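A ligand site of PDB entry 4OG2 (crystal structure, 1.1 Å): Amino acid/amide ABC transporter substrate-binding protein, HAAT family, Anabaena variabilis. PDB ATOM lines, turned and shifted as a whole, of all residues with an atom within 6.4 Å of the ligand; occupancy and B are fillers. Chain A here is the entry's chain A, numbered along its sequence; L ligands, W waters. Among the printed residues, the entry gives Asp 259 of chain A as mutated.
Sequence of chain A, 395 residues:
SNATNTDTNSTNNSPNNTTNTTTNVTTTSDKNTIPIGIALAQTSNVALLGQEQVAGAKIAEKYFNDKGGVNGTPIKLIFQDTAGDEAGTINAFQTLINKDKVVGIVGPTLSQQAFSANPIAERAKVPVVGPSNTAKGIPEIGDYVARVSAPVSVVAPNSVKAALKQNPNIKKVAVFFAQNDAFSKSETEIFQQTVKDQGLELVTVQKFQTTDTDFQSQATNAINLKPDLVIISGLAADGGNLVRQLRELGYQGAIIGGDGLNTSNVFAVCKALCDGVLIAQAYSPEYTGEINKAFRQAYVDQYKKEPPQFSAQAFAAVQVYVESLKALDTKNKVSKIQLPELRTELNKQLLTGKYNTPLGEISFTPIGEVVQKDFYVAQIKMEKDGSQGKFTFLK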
ATOM      1  N   LEU A  49      30.309  21.355 -13.704  1.00  0.00           N
ATOM      2  CA  LEU A  49      28.982  20.857 -13.355  1.00  0.00           C
ATOM      3  C   LEU A  49      28.404  20.051 -14.527  1.00  0.00           C
ATOM      4  O   LEU A  49      27.842  18.958 -14.335  1.00  0.00           O
ATOM      5  CB  LEU A  49      28.077  22.040 -12.997  1.00  0.00           C
ATOM      6  CG  LEU A  49      28.634  22.872 -11.839  1.00  0.00           C
ATOM      7  CD1 LEU A  49      28.065  24.285 -11.796  1.00  0.00           C
ATOM      8  CD2 LEU A  49      28.440  22.172 -10.499  1.00  0.00           C
ATOM      9  N   GLY A  50      28.545  20.578 -15.746  1.00  0.00           N
ATOM     10  CA  GLY A  50      27.955  19.955 -16.913  1.00  0.00           C
ATOM     11  C   GLY A  50      28.455  18.569 -17.231  1.00  0.00           C
ATOM     12  O   GLY A  50      27.696  17.740 -17.727  1.00  0.00           O
ATOM     13  N   GLN A  53      26.454  15.849 -15.833  1.00  0.00           N
ATOM     14  CA  GLN A  53      25.178  15.741 -16.503  1.00  0.00           C
ATOM     15  C   GLN A  53      25.314  14.950 -17.788  1.00  0.00           C
ATOM     16  O   GLN A  53      24.500  14.088 -18.095  1.00  0.00           O
ATOM     17  CB  GLN A  53      24.618  17.134 -16.782  1.00  0.00           C
ATOM     18  CG  GLN A  53      24.394  17.941 -15.532  1.00  0.00           C
ATOM     19  CD  GLN A  53      23.886  19.312 -15.862  1.00  0.00           C
ATOM     20  OE1 GLN A  53      24.485  20.026 -16.662  1.00  0.00           O
ATOM     21  NE2 GLN A  53      22.773  19.692 -15.261  1.00  0.00           N
ATOM     22  N   THR A 109      22.558  23.763 -18.490  1.00  0.00           N
ATOM     23  CA  THR A 109      23.114  23.477 -17.185  1.00  0.00           C
ATOM     24  C   THR A 109      22.678  24.499 -16.129  1.00  0.00           C
ATOM     25  O   THR A 109      22.280  24.142 -15.023  1.00  0.00           O
ATOM     26  CB  THR A 109      24.655  23.387 -17.255  1.00  0.00           C
ATOM     27  OG1 THR A 109      25.017  22.293 -18.096  1.00  0.00           O
ATOM     28  CG2 THR A 109      25.284  23.212 -15.863  1.00  0.00           C
ATOM     29  N   LEU A 110      22.779  25.786 -16.463  1.00  0.00           N
ATOM     30  CA  LEU A 110      22.551  26.843 -15.470  1.00  0.00           C
ATOM     31  C   LEU A 110      21.216  27.555 -15.642  1.00  0.00           C
ATOM     32  O   LEU A 110      20.793  27.848 -16.766  1.00  0.00           O
ATOM     33  CB  LEU A 110      23.636  27.926 -15.569  1.00  0.00           C
ATOM     34  CG  LEU A 110      25.058  27.473 -15.280  1.00  0.00           C
ATOM     35  CD1 LEU A 110      25.993  28.651 -15.452  1.00  0.00           C
ATOM     36  CD2 LEU A 110      25.181  26.867 -13.883  1.00  0.00           C
ATOM     37  N   SER A 111      20.584  27.913 -14.528  1.00  0.00           N
ATOM     38  CA  SER A 111      19.427  28.802 -14.574  1.00  0.00           C
ATOM     39  C   SER A 111      19.755  30.127 -15.278  1.00  0.00           C
ATOM     40  O   SER A 111      18.926  30.648 -16.020  1.00  0.00           O
ATOM     41  CB  SER A 111      18.908  29.109 -13.172  1.00  0.00           C
ATOM     42  OG  SER A 111      18.354  27.961 -12.554  1.00  0.00           O
ATOM     43  N   GLN A 112      20.954  30.656 -15.051  1.00  0.00           N
ATOM     44  CA  GLN A 112      21.387  31.885 -15.727  1.00  0.00           C
ATOM     45  C   GLN A 112      21.224  31.761 -17.239  1.00  0.00           C
ATOM     46  O   GLN A 112      20.785  32.701 -17.909  1.00  0.00           O
ATOM     47  CB  GLN A 112      22.853  32.152 -15.398  1.00  0.00           C
ATOM     48  CG  GLN A 112      23.434  33.384 -16.099  1.00  0.00           C
ATOM     49  CD  GLN A 112      22.879  34.691 -15.555  1.00  0.00           C
ATOM     50  OE1 GLN A 112      22.524  34.784 -14.379  1.00  0.00           O
ATOM     51  NE2 GLN A 112      22.799  35.687 -16.415  1.00  0.00           N
ATOM     52  N   SER A 132      18.738  20.285 -13.861  1.00  0.00           N
ATOM     53  CA  SER A 132      19.289  20.688 -12.562  1.00  0.00           C
ATOM     54  C   SER A 132      19.090  22.166 -12.264  1.00  0.00           C
ATOM     55  O   SER A 132      19.606  22.648 -11.260  1.00  0.00           O
ATOM     56  CB  SER A 132      20.776  20.347 -12.485  1.00  0.00           C
ATOM     57  OG  SER A 132      21.002  18.995 -12.858  1.00  0.00           O
ATOM     58  N   ASN A 133      18.353  22.875 -13.117  1.00  0.00           N
ATOM     59  CA  ASN A 133      18.151  24.303 -12.884  1.00  0.00           C
ATOM     60  C   ASN A 133      17.066  24.570 -11.853  1.00  0.00           C
ATOM     61  O   ASN A 133      15.917  24.156 -12.017  1.00  0.00           O
ATOM     62  CB  ASN A 133      17.991  25.145 -14.159  1.00  0.00           C
ATOM     63  CG  ASN A 133      16.962  24.579 -15.130  1.00  0.00           C
ATOM     64  OD1 ASN A 133      16.007  23.892 -14.755  1.00  0.00           O
ATOM     65  ND2 ASN A 133      17.162  24.901 -16.417  1.00  0.00           N
ATOM     66  N   THR A 134      17.472  25.270 -10.798  1.00  0.00           N
ATOM     67  CA  THR A 134      16.710  25.305  -9.560  1.00  0.00           C
ATOM     68  C   THR A 134      16.311  26.702  -9.088  1.00  0.00           C
ATOM     69  O   THR A 134      15.727  26.847  -8.013  1.00  0.00           O
ATOM     70  CB  THR A 134      17.456  24.540  -8.437  1.00  0.00           C
ATOM     71  OG1 THR A 134      18.726  25.156  -8.225  1.00  0.00           O
ATOM     72  CG2 THR A 134      17.632  23.068  -8.827  1.00  0.00           C
ATOM     73  N   ALA A 135      16.601  27.727  -9.880  1.00  0.00           N
ATOM     74  CA  ALA A 135      16.177  29.083  -9.543  1.00  0.00           C
ATOM     75  C   ALA A 135      14.651  29.204  -9.558  1.00  0.00           C
ATOM     76  O   ALA A 135      13.947  28.538 -10.330  1.00  0.00           O
ATOM     77  CB  ALA A 135      16.762  30.088 -10.508  1.00  0.00           C
ATOM     78  N   ILE A 138      11.746  29.204 -13.156  1.00  0.00           N
ATOM     79  CA  ILE A 138      12.082  28.473 -14.386  1.00  0.00           C
ATOM     80  C   ILE A 138      10.857  27.885 -15.120  1.00  0.00           C
ATOM     81  O   ILE A 138      10.669  28.167 -16.300  1.00  0.00           O
ATOM     82  CB  ILE A 138      13.185  27.422 -14.130  1.00  0.00           C
ATOM     83  CG1 ILE A 138      14.516  28.095 -13.766  1.00  0.00           C
ATOM     84  CG2 ILE A 138      13.336  26.501 -15.331  1.00  0.00           C
ATOM     85  CD1 ILE A 138      15.284  28.604 -14.961  1.00  0.00           C
ATOM     86  N   SER A 149      14.361  19.043 -11.616  1.00  0.00           N
ATOM     87  CA  SER A 149      15.170  19.435 -10.464  1.00  0.00           C
ATOM     88  C   SER A 149      14.390  20.321  -9.533  1.00  0.00           C
ATOM     89  O   SER A 149      14.035  21.454  -9.879  1.00  0.00           O
ATOM     90  CB  SER A 149      16.401  20.191 -10.938  1.00  0.00           C
ATOM     91  OG  SER A 149      16.052  21.257 -11.807  1.00  0.00           O
ATOM     92  N   VAL A 152      15.352  25.685  -5.311  1.00  0.00           N
ATOM     93  CA  VAL A 152      16.099  26.104  -4.137  1.00  0.00           C
ATOM     94  C   VAL A 152      15.239  26.204  -2.863  1.00  0.00           C
ATOM     95  O   VAL A 152      15.704  25.900  -1.774  1.00  0.00           O
ATOM     96  CB  VAL A 152      16.845  27.445  -4.374  1.00  0.00           C
ATOM     97  CG1 VAL A 152      17.976  27.247  -5.386  1.00  0.00           C
ATOM     98  CG2 VAL A 152      15.896  28.547  -4.836  1.00  0.00           C
ATOM     99  N   ASP A 181      25.139  35.538 -10.987  1.00  0.00           N
ATOM    100  CA  ASP A 181      24.523  34.273 -11.366  1.00  0.00           C
ATOM    101  C   ASP A 181      23.095  34.142 -10.836  1.00  0.00           C
ATOM    102  O   ASP A 181      22.845  34.260  -9.630  1.00  0.00           O
ATOM    103  CB  ASP A 181      25.385  33.105 -10.866  1.00  0.00           C
ATOM    104  CG  ASP A 181      24.759  31.767 -11.176  1.00  0.00           C
ATOM    105  OD1 ASP A 181      24.784  31.363 -12.355  1.00  0.00           O
ATOM    106  OD2 ASP A 181      24.217  31.137 -10.250  1.00  0.00           O
ATOM    107  N   ALA A 182      22.156  33.889 -11.738  1.00  0.00           N
ATOM    108  CA  ALA A 182      20.737  33.920 -11.374  1.00  0.00           C
ATOM    109  C   ALA A 182      20.391  32.905 -10.295  1.00  0.00           C
ATOM    110  O   ALA A 182      19.636  33.206  -9.365  1.00  0.00           O
ATOM    111  CB  ALA A 182      19.864  33.704 -12.594  1.00  0.00           C
ATOM    112  N   PHE A 183      20.893  31.686 -10.431  1.00  0.00           N
ATOM    113  CA  PHE A 183      20.612  30.658  -9.431  1.00  0.00           C
ATOM    114  C   PHE A 183      21.202  31.021  -8.085  1.00  0.00           C
ATOM    115  O   PHE A 183      20.566  30.829  -7.059  1.00  0.00           O
ATOM    116  CB  PHE A 183      21.097  29.288  -9.927  1.00  0.00           C
ATOM    117  CG  PHE A 183      21.683  28.430  -8.836  1.00  0.00           C
ATOM    118  CD1 PHE A 183      20.873  27.666  -8.006  1.00  0.00           C
ATOM    119  CD2 PHE A 183      23.054  28.393  -8.660  1.00  0.00           C
ATOM    120  CE1 PHE A 183      21.439  26.907  -7.001  1.00  0.00           C
ATOM    121  CE2 PHE A 183      23.616  27.631  -7.668  1.00  0.00           C
ATOM    122  CZ  PHE A 183      22.817  26.891  -6.822  1.00  0.00           C
ATOM    123  N   SER A 184      22.419  31.564  -8.076  1.00  0.00           N
ATOM    124  CA  SER A 184      23.077  31.894  -6.807  1.00  0.00           C
ATOM    125  C   SER A 184      22.292  32.958  -6.061  1.00  0.00           C
ATOM    126  O   SER A 184      22.157  32.899  -4.839  1.00  0.00           O
ATOM    127  CB  SER A 184      24.506  32.366  -7.055  1.00  0.00           C
ATOM    128  OG  SER A 184      25.301  31.328  -7.605  1.00  0.00           O
ATOM    129  N   GLY A 234      27.536  29.808  -4.905  1.00  0.00           N
ATOM    130  CA  GLY A 234      28.247  30.113  -6.138  1.00  0.00           C
ATOM    131  C   GLY A 234      28.266  28.868  -6.989  1.00  0.00           C
ATOM    132  O   GLY A 234      27.448  27.968  -6.809  1.00  0.00           O
ATOM    133  N   LEU A 235      29.198  28.829  -7.935  1.00  0.00           N
ATOM    134  CA  LEU A 235      29.426  27.636  -8.725  1.00  0.00           C
ATOM    135  C   LEU A 235      30.675  26.910  -8.201  1.00  0.00           C
ATOM    136  O   LEU A 235      31.101  27.107  -7.054  1.00  0.00           O
ATOM    137  CB  LEU A 235      29.431  27.949 -10.225  1.00  0.00           C
ATOM    138  CG  LEU A 235      28.129  28.625 -10.694  1.00  0.00           C
ATOM    139  CD1 LEU A 235      28.206  28.938 -12.180  1.00  0.00           C
ATOM    140  CD2 LEU A 235      26.881  27.786 -10.382  1.00  0.00           C
ATOM    141  N   ASP A 259      24.049  24.369  -4.257  1.00  0.00           N
ATOM    142  CA  ASP A 259      24.028  23.367  -5.315  1.00  0.00           C
ATOM    143  C   ASP A 259      25.219  23.507  -6.275  1.00  0.00           C
ATOM    144  O   ASP A 259      25.653  22.524  -6.871  1.00  0.00           O
ATOM    145  CB  ASP A 259      22.711  23.474  -6.090  1.00  0.00           C
ATOM    146  CG  ASP A 259      22.327  22.198  -6.832  1.00  0.00           C
ATOM    147  OD1 ASP A 259      22.397  21.107  -6.232  1.00  0.00           O
ATOM    148  OD2 ASP A 259      21.899  22.301  -8.013  1.00  0.00           O
ATOM    149  N   GLY A 260      25.741  24.722  -6.428  1.00  0.00           N
ATOM    150  CA  GLY A 260      26.846  24.941  -7.336  1.00  0.00           C
ATOM    151  C   GLY A 260      28.157  24.344  -6.891  1.00  0.00           C
ATOM    152  O   GLY A 260      29.093  24.224  -7.682  1.00  0.00           O
ATOM    153  N   LEU A 261      28.237  23.972  -5.602  1.00  0.00           N
ATOM    154  CA  LEU A 261      29.426  23.302  -5.069  1.00  0.00           C
ATOM    155  C   LEU A 261      29.231  21.787  -5.005  1.00  0.00           C
ATOM    156  O   LEU A 261      30.116  21.062  -4.548  1.00  0.00           O
ATOM    157  CB  LEU A 261      29.768  23.826  -3.672  1.00  0.00           C
ATOM    158  CG  LEU A 261      30.399  25.213  -3.611  1.00  0.00           C
ATOM    159  CD1 LEU A 261      29.389  26.325  -3.868  1.00  0.00           C
ATOM    160  CD2 LEU A 261      31.077  25.403  -2.265  1.00  0.00           C
ATOM    161  N   ASN A 262      28.099  21.310  -5.517  1.00  0.00           N
ATOM    162  CA  ASN A 262      27.712  19.907  -5.359  1.00  0.00           C
ATOM    163  C   ASN A 262      28.342  18.999  -6.412  1.00  0.00           C
ATOM    164  O   ASN A 262      27.655  18.382  -7.213  1.00  0.00           O
ATOM    165  CB  ASN A 262      26.190  19.794  -5.389  1.00  0.00           C
ATOM    166  CG  ASN A 262      25.694  18.458  -4.863  1.00  0.00           C
ATOM    167  OD1 ASN A 262      26.447  17.696  -4.268  1.00  0.00           O
ATOM    168  ND2 ASN A 262      24.413  18.174  -5.082  1.00  0.00           N
ATOM    169  N   GLN A 309      24.342  13.615  -7.788  1.00  0.00           N
ATOM    170  CA  GLN A 309      23.052  14.214  -8.076  1.00  0.00           C
ATOM    171  C   GLN A 309      22.876  14.654  -9.533  1.00  0.00           C
ATOM    172  O   GLN A 309      21.871  14.338 -10.171  1.00  0.00           O
ATOM    173  CB  GLN A 309      22.819  15.402  -7.163  1.00  0.00           C
ATOM    174  CG  GLN A 309      21.515  16.126  -7.421  1.00  0.00           C
ATOM    175  CD  GLN A 309      21.467  17.433  -6.692  1.00  0.00           C
ATOM    176  OE1 GLN A 309      21.232  17.463  -5.483  1.00  0.00           O
ATOM    177  NE2 GLN A 309      21.744  18.529  -7.395  1.00  0.00           N
ATOM    178  N   PHE A 310      23.858  15.395 -10.068  1.00  0.00           N
ATOM    179  CA  PHE A 310      23.681  15.951 -11.410  1.00  0.00           C
ATOM    180  C   PHE A 310      23.580  14.867 -12.482  1.00  0.00           C
ATOM    181  O   PHE A 310      22.864  15.033 -13.478  1.00  0.00           O
ATOM    182  CB  PHE A 310      24.784  16.965 -11.743  1.00  0.00           C
ATOM    183  CG  PHE A 310      24.740  18.198 -10.882  1.00  0.00           C
ATOM    184  CD1 PHE A 310      23.524  18.835 -10.636  1.00  0.00           C
ATOM    185  CD2 PHE A 310      25.877  18.698 -10.278  1.00  0.00           C
ATOM    186  CE1 PHE A 310      23.459  19.966  -9.835  1.00  0.00           C
ATOM    187  CE2 PHE A 310      25.804  19.831  -9.459  1.00  0.00           C
ATOM    188  CZ  PHE A 310      24.585  20.453  -9.248  1.00  0.00           C
HETATM  189  N1  LIG L   1      21.140  24.460  -9.797  1.00  0.00           N
HETATM  190  C1  LIG L   1      22.033  25.321 -10.579  1.00  0.00           C
HETATM  191  C2  LIG L   1      21.255  26.351 -11.352  1.00  0.00           C
HETATM  192  O1  LIG L   1      20.017  26.390 -11.233  1.00  0.00           O
HETATM  193  C3  LIG L   1      22.872  24.516 -11.564  1.00  0.00           C
HETATM  194  C4  LIG L   1      23.685  23.374 -10.978  1.00  0.00           C
HETATM  195  C5  LIG L   1      24.390  22.647 -12.106  1.00  0.00           C
HETATM  196  C6  LIG L   1      24.663  23.912  -9.940  1.00  0.00           C
HETATM  197  O2  LIG L   1      21.884  27.126 -12.097  1.00  0.00           O
HETATM  198  O   HOH W   1      22.594  29.887 -12.851  1.00  0.00           O
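N of Ser 111 sits at hydrogen-bond distance from O2 of the ligand, 2.9 Å away. An oxygen (O1) of the ligand lies within hydrogen-bond range of the side-chain hydroxyl of Ser 111, at 2.6 Å. OG1 of Thr 134 is in hydrogen-bond range of N1 of the ligand. O of Ser 132 is in hydrogen-bond range of N1 of the ligand (2.8 Å). The backbone NH of Thr 134 lies within hydrogen-bond range of an oxygen (O1) of the ligand (2.8 Å). The side-chain carboxylate of Asp 259 is in salt-bridge range of a nitrogen (N1) of the ligand (2.9 Å).
The backbone NH of Val 152 lies within hydrogen-bond range of the backbone carbonyl oxygen of Thr 134 (3.0 Å). OG of Ser 132 lies within hydrogen-bond range of NE2 of Gln 53, at 3.1 Å. The side-chain carboxylate (OD1) of Asp 259 lies within hydrogen-bond range of the side-chain amide nitrogen (NE2) of Gln 309 (2.9 Å). N of Phe 183 lies close to OD2 of Asp 181 (3.4 Å). The side-chain hydroxyl (OG) of Ser 111 lies within hydrogen-bond range of the backbone NH (N) of Ala 135, at 3.2 Å. OG of Ser 149 sits at hydrogen-bond distance from O of Asn 133, at 2.9 Å. The side-chain hydroxyl of Thr 109 is in hydrogen-bond range of the side-chain amide oxygen of Gln 53. The side-chain hydroxyl (OG) of Ser 111 lies within hydrogen-bond range of the backbone NH (N) of Thr 134.
Residues that only touch the ligand: Leu 49 (3.8 Å), Thr 109 (3.5 Å), Leu 110 (3.4 Å), Asn 133 (3.3 Å), Ala 135 (3.9 Å), Phe 183 (3.2 Å), Gly 260 (3.6 Å) and Phe 310 (3.5 Å). Of the 26 residues printed, 12 come within 4 Å of the ligand.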
